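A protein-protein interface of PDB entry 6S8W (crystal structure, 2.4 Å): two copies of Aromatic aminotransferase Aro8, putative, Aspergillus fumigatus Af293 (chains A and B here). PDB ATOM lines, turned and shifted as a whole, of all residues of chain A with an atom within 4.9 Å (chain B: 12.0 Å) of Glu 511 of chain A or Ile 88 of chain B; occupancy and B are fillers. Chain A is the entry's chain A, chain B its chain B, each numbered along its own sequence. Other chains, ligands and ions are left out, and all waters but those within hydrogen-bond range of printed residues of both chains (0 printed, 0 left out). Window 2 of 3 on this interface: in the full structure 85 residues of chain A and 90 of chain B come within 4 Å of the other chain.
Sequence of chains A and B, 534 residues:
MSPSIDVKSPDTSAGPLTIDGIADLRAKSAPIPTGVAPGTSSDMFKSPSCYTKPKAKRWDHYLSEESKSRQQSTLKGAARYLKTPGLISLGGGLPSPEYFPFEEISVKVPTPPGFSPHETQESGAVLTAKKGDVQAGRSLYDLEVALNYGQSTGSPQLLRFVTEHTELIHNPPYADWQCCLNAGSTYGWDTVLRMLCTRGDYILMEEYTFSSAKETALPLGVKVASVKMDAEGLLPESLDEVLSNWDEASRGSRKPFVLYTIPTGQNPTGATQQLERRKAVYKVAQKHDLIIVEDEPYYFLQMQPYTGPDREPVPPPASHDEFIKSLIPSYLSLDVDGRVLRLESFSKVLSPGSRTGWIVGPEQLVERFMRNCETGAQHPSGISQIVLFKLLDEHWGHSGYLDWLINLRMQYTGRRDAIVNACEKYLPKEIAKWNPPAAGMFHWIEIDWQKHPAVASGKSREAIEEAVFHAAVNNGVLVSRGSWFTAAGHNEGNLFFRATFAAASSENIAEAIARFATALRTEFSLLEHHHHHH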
ATOM      1  N   GLY A 476      -4.331  21.187 -26.412  1.00  0.00           N
ATOM      2  CA  GLY A 476      -5.409  21.294 -27.413  1.00  0.00           C
ATOM      3  C   GLY A 476      -6.719  20.706 -26.915  1.00  0.00           C
ATOM      4  O   GLY A 476      -7.412  20.052 -27.721  1.00  0.00           O
ATOM      5  N   VAL A 477      -7.052  20.927 -25.638  1.00  0.00           N
ATOM      6  CA  VAL A 477      -8.420  20.700 -25.081  1.00  0.00           C
ATOM      7  C   VAL A 477      -8.889  21.995 -24.412  1.00  0.00           C
ATOM      8  O   VAL A 477      -8.117  22.567 -23.619  1.00  0.00           O
ATOM      9  CB  VAL A 477      -8.480  19.515 -24.096  1.00  0.00           C
ATOM     10  CG1 VAL A 477      -7.559  19.708 -22.903  1.00  0.00           C
ATOM     11  CG2 VAL A 477      -9.905  19.260 -23.627  1.00  0.00           C
ATOM     12  N   LEU A 478     -10.105  22.436 -24.740  1.00  0.00           N
ATOM     13  CA  LEU A 478     -10.778  23.601 -24.106  1.00  0.00           C
ATOM     14  C   LEU A 478     -11.866  23.099 -23.151  1.00  0.00           C
ATOM     15  O   LEU A 478     -12.700  22.277 -23.582  1.00  0.00           O
ATOM     16  CB  LEU A 478     -11.379  24.493 -25.198  1.00  0.00           C
ATOM     17  N   GLU A 507     -15.413   9.501 -30.025  1.00  0.00           N
ATOM     18  CA  GLU A 507     -13.946   9.471 -30.272  1.00  0.00           C
ATOM     19  C   GLU A 507     -13.297  10.692 -29.610  1.00  0.00           C
ATOM     20  O   GLU A 507     -12.347  10.502 -28.827  1.00  0.00           O
ATOM     21  CB  GLU A 507     -13.639   9.468 -31.772  1.00  0.00           C
ATOM     22  CG  GLU A 507     -14.338   8.362 -32.540  1.00  0.00           C
ATOM     23  CD  GLU A 507     -15.698   8.742 -33.098  1.00  0.00           C
ATOM     24  OE1 GLU A 507     -15.763   9.711 -33.878  1.00  0.00           O
ATOM     25  OE2 GLU A 507     -16.688   8.068 -32.751  1.00  0.00           O
ATOM     26  N   ASN A 508     -13.800  11.893 -29.919  1.00  0.00           N
ATOM     27  CA  ASN A 508     -13.226  13.194 -29.479  1.00  0.00           C
ATOM     28  C   ASN A 508     -13.446  13.383 -27.973  1.00  0.00           C
ATOM     29  O   ASN A 508     -12.631  14.088 -27.349  1.00  0.00           O
ATOM     30  CB  ASN A 508     -13.820  14.370 -30.258  1.00  0.00           C
ATOM     31  CG  ASN A 508     -13.263  14.493 -31.660  1.00  0.00           C
ATOM     32  OD1 ASN A 508     -12.597  13.583 -32.150  1.00  0.00           O
ATOM     33  ND2 ASN A 508     -13.536  15.608 -32.318  1.00  0.00           N
ATOM     34  N   ILE A 509     -14.507  12.789 -27.419  1.00  0.00           N
ATOM     35  CA  ILE A 509     -14.843  12.869 -25.965  1.00  0.00           C
ATOM     36  C   ILE A 509     -13.705  12.224 -25.166  1.00  0.00           C
ATOM     37  O   ILE A 509     -13.214  12.869 -24.220  1.00  0.00           O
ATOM     38  CB  ILE A 509     -16.204  12.209 -25.669  1.00  0.00           C
ATOM     39  CG1 ILE A 509     -16.672  12.498 -24.240  1.00  0.00           C
ATOM     40  N   ALA A 510     -13.305  11.004 -25.538  1.00  0.00           N
ATOM     41  CA  ALA A 510     -12.167  10.270 -24.932  1.00  0.00           C
ATOM     42  C   ALA A 510     -10.886  11.089 -25.125  1.00  0.00           C
ATOM     43  O   ALA A 510     -10.310  11.541 -24.115  1.00  0.00           O
ATOM     44  CB  ALA A 510     -12.049   8.897 -25.546  1.00  0.00           C
ATOM     45  N   GLU A 511     -10.471  11.272 -26.382  1.00  0.00           N
ATOM     46  CA  GLU A 511      -9.308  12.104 -26.795  1.00  0.00           C
ATOM     47  C   GLU A 511      -9.217  13.343 -25.902  1.00  0.00           C
ATOM     48  O   GLU A 511      -8.181  13.506 -25.220  1.00  0.00           O
ATOM     49  CB  GLU A 511      -9.455  12.496 -28.266  1.00  0.00           C
ATOM     50  CG  GLU A 511      -8.452  13.537 -28.732  1.00  0.00           C
ATOM     51  CD  GLU A 511      -7.034  13.022 -28.909  1.00  0.00           C
ATOM     52  OE1 GLU A 511      -6.858  11.789 -28.975  1.00  0.00           O
ATOM     53  OE2 GLU A 511      -6.110  13.856 -28.982  1.00  0.00           O
ATOM     54  N   ALA A 512     -10.255  14.186 -25.911  1.00  0.00           N
ATOM     55  CA  ALA A 512     -10.326  15.461 -25.156  1.00  0.00           C
ATOM     56  C   ALA A 512     -10.013  15.218 -23.675  1.00  0.00           C
ATOM     57  O   ALA A 512      -9.208  15.989 -23.115  1.00  0.00           O
ATOM     58  CB  ALA A 512     -11.683  16.095 -25.334  1.00  0.00           C
ATOM     59  N   ILE A 513     -10.625  14.199 -23.061  1.00  0.00           N
ATOM     60  CA  ILE A 513     -10.429  13.862 -21.619  1.00  0.00           C
ATOM     61  C   ILE A 513      -8.966  13.446 -21.412  1.00  0.00           C
ATOM     62  O   ILE A 513      -8.345  13.920 -20.439  1.00  0.00           O
ATOM     63  CB  ILE A 513     -11.415  12.770 -21.153  1.00  0.00           C
ATOM     64  CG1 ILE A 513     -12.846  13.307 -21.063  1.00  0.00           C
ATOM     65  CG2 ILE A 513     -10.963  12.162 -19.830  1.00  0.00           C
ATOM     66  CD1 ILE A 513     -13.055  14.319 -19.960  1.00  0.00           C
ATOM     67  N   ALA A 514      -8.446  12.602 -22.309  1.00  0.00           N
ATOM     68  CA  ALA A 514      -7.052  12.102 -22.308  1.00  0.00           C
ATOM     69  C   ALA A 514      -6.078  13.282 -22.377  1.00  0.00           C
ATOM     70  O   ALA A 514      -5.053  13.246 -21.669  1.00  0.00           O
ATOM     71  CB  ALA A 514      -6.843  11.151 -23.460  1.00  0.00           C
ATOM     72  N   ARG A 515      -6.386  14.284 -23.204  1.00  0.00           N
ATOM     73  CA  ARG A 515      -5.541  15.493 -23.386  1.00  0.00           C
ATOM     74  C   ARG A 515      -5.496  16.284 -22.083  1.00  0.00           C
ATOM     75  O   ARG A 515      -4.468  16.935 -21.810  1.00  0.00           O
ATOM     76  CB  ARG A 515      -6.117  16.416 -24.456  1.00  0.00           C
ATOM     77  CG  ARG A 515      -6.108  15.822 -25.852  1.00  0.00           C
ATOM     78  CD  ARG A 515      -5.992  16.941 -26.856  1.00  0.00           C
ATOM     79  NE  ARG A 515      -6.031  16.414 -28.204  1.00  0.00           N
ATOM     80  CZ  ARG A 515      -6.464  17.092 -29.253  1.00  0.00           C
ATOM     81  NH1 ARG A 515      -6.901  18.330 -29.101  1.00  0.00           N
ATOM     82  NH2 ARG A 515      -6.464  16.528 -30.446  1.00  0.00           N
ATOM     83  N   GLY B  86      -6.369  24.569 -34.400  1.00  0.00           N
ATOM     84  CA  GLY B  86      -7.597  23.759 -34.296  1.00  0.00           C
ATOM     85  C   GLY B  86      -7.497  22.741 -33.178  1.00  0.00           C
ATOM     86  O   GLY B  86      -6.601  21.885 -33.240  1.00  0.00           O
ATOM     87  N   LEU B  87      -8.379  22.828 -32.181  1.00  0.00           N
ATOM     88  CA  LEU B  87      -8.400  21.894 -31.029  1.00  0.00           C
ATOM     89  C   LEU B  87      -9.837  21.470 -30.729  1.00  0.00           C
ATOM     90  O   LEU B  87     -10.778  22.058 -31.308  1.00  0.00           O
ATOM     91  CB  LEU B  87      -7.774  22.579 -29.812  1.00  0.00           C
ATOM     92  CG  LEU B  87      -8.439  23.888 -29.394  1.00  0.00           C
ATOM     93  CD1 LEU B  87      -9.650  23.625 -28.512  1.00  0.00           C
ATOM     94  CD2 LEU B  87      -7.444  24.787 -28.681  1.00  0.00           C
ATOM     95  N   ILE B  88      -9.974  20.500 -29.826  1.00  0.00           N
ATOM     96  CA  ILE B  88     -11.266  19.880 -29.425  1.00  0.00           C
ATOM     97  C   ILE B  88     -11.838  20.703 -28.266  1.00  0.00           C
ATOM     98  O   ILE B  88     -11.087  20.998 -27.316  1.00  0.00           O
ATOM     99  CB  ILE B  88     -11.054  18.392 -29.075  1.00  0.00           C
ATOM    100  CG1 ILE B  88     -10.217  17.677 -30.142  1.00  0.00           C
ATOM    101  CG2 ILE B  88     -12.382  17.688 -28.846  1.00  0.00           C
ATOM    102  CD1 ILE B  88      -9.667  16.335 -29.708  1.00  0.00           C
ATOM    103  N   SER B  89     -13.107  21.100 -28.372  1.00  0.00           N
ATOM    104  CA  SER B  89     -13.820  21.917 -27.356  1.00  0.00           C
ATOM    105  C   SER B  89     -14.844  21.058 -26.608  1.00  0.00           C
ATOM    106  O   SER B  89     -15.673  20.406 -27.274  1.00  0.00           O
ATOM    107  CB  SER B  89     -14.482  23.114 -27.986  1.00  0.00           C
ATOM    108  OG  SER B  89     -15.402  23.719 -27.087  1.00  0.00           O
ATOM    109  N   LEU B  90     -14.772  21.063 -25.275  1.00  0.00           N
ATOM    110  CA  LEU B  90     -15.865  20.621 -24.367  1.00  0.00           C
ATOM    111  C   LEU B  90     -16.334  21.840 -23.564  1.00  0.00           C
ATOM    112  O   LEU B  90     -16.697  21.669 -22.384  1.00  0.00           O
ATOM    113  CB  LEU B  90     -15.359  19.513 -23.437  1.00  0.00           C
ATOM    114  CG  LEU B  90     -14.646  18.338 -24.105  1.00  0.00           C
ATOM    115  CD1 LEU B  90     -14.410  17.218 -23.102  1.00  0.00           C
ATOM    116  CD2 LEU B  90     -15.429  17.821 -25.302  1.00  0.00           C
ATOM    117  N   GLY B  91     -16.329  23.020 -24.194  1.00  0.00           N
ATOM    118  CA  GLY B  91     -16.436  24.329 -23.518  1.00  0.00           C
ATOM    119  C   GLY B  91     -17.860  24.858 -23.466  1.00  0.00           C
ATOM    120  O   GLY B  91     -18.313  25.204 -22.358  1.00  0.00           O
ATOM    121  N   GLY B  92     -18.543  24.925 -24.615  1.00  0.00           N
ATOM    122  CA  GLY B  92     -19.844  25.610 -24.767  1.00  0.00           C
ATOM    123  C   GLY B  92     -21.018  24.645 -24.763  1.00  0.00           C
ATOM    124  O   GLY B  92     -20.791  23.437 -24.962  1.00  0.00           O
ATOM    125  N   GLY B  93     -22.236  25.163 -24.567  1.00  0.00           N
ATOM    126  CA  GLY B  93     -23.468  24.375 -24.365  1.00  0.00           C
ATOM    127  C   GLY B  93     -24.282  24.221 -25.640  1.00  0.00           C
ATOM    128  O   GLY B  93     -25.499  23.981 -25.531  1.00  0.00           O
ATOM    129  N   LEU B  94     -23.639  24.348 -26.805  1.00  0.00           N
ATOM    130  CA  LEU B  94     -24.276  24.176 -28.141  1.00  0.00           C
ATOM    131  C   LEU B  94     -24.601  22.702 -28.364  1.00  0.00           C
ATOM    132  O   LEU B  94     -23.702  21.866 -28.401  1.00  0.00           O
ATOM    133  CB  LEU B  94     -23.317  24.676 -29.225  1.00  0.00           C
ATOM    134  CG  LEU B  94     -23.393  26.164 -29.560  1.00  0.00           C
ATOM    135  CD1 LEU B  94     -23.615  27.003 -28.312  1.00  0.00           C
ATOM    136  CD2 LEU B  94     -22.135  26.610 -30.288  1.00  0.00           C
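No position is printed for both chains.
Hydrophobic or aromatic side chains of chain B within 4 Å of the printed part of chain A: Leu 87, Ile 88 and Leu 90. Of the 12 printed residues of chain A, 7 touch a printed residue of chain B. Among the printed residues, no Asp or Glu carboxylate lies within 4 Å of a Lys or Arg side-chain nitrogen of the other chain.
The backbone NH of Ile 88 of chain B lies within hydrogen-bond range of the backbone carbonyl oxygen of Gly 476 of chain A. N of Leu 478 of chain A sits at hydrogen-bond distance from O of Ile 88 of chain B. O of Leu 478 of chain A lies within hydrogen-bond range of N of Leu 90 of chain B, at 2.9 Å.
The side-chain carboxylate of Glu 511 of chain A lies within salt-bridge range of the guanidinium group of Arg 515 of chain A. The backbone NH of Gly 91 of chain B sits at hydrogen-bond distance from the side-chain hydroxyl of Ser 89 of chain B (3.1 Å).
Printed residues of chain B within 4 Å of Leu 478 of chain A: Leu 87 (3.8 Å), Ile 88 (3.1 Å), Ser 89 (3.9 Å), Leu 90 (2.9 Å) and Gly 91 (3.8 Å). No residue of chain B comes within 4 Å of Ala 510 of chain A. Ala 512 of chain A touches just these residues of chain B: Ile 88 and Leu 90. No residue of chain B comes within 4 Å of Ile 513 of chain A. Printed residues of chain A within 4 Å of Leu 87 of chain B: Gly 476 (3.3 Å) and Leu 478 (3.8 Å). Printed residues of chain A within 4 Å of Ile 88 of chain B: Gly 476 (3.3 Å), Val 477 (3.5 Å), Leu 478 (3.1 Å), Asn 508 (3.9 Å), Glu 511 (3.2 Å), Ala 512 (3.9 Å) and Arg 515 (3.3 Å). Of the printed residues of chain A, Ser 89 of chain B touches Leu 478 (3.9 Å). Printed residues of chain A within 4 Å of Leu 90 of chain B: Leu 478 (2.9 Å) and Ala 512 (3.7 Å). Printed residues of chain A within 4 Å of Gly 91 of chain B: Leu 478. Gly 93 of chain B touches none of the printed residues of chain A. Leu 94 of chain B touches none of the printed residues of chain A. The nearest residue of chain B that does not touch Glu 511 of chain A is Leu 90 of chain B (7.1 Å).
Among the printed residues, merely in contact across the chains: Glu 511 of chain A with Ile 88 of chain B (3.2 Å), Arg 515 of chain A with Ile 88 of chain B (3.3 Å), Gly 476 of chain A with Leu 87 of chain B (3.3 Å), Val 477 of chain A with Ile 88 of chain B (3.5 Å), Ala 512 of chain A with Leu 90 of chain B (3.7 Å), Leu 478 of chain A with Gly 91 of chain B (3.8 Å), Leu 478 of chain A with Leu 87 of chain B (3.8 Å), Asn 508 of chain A with Ile 88 of chain B (3.9 Å), Leu 478 of chain A with Ser 89 of chain B (3.9 Å) and Ala 512 of chain A with Ile 88 of chain B (3.9 Å).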
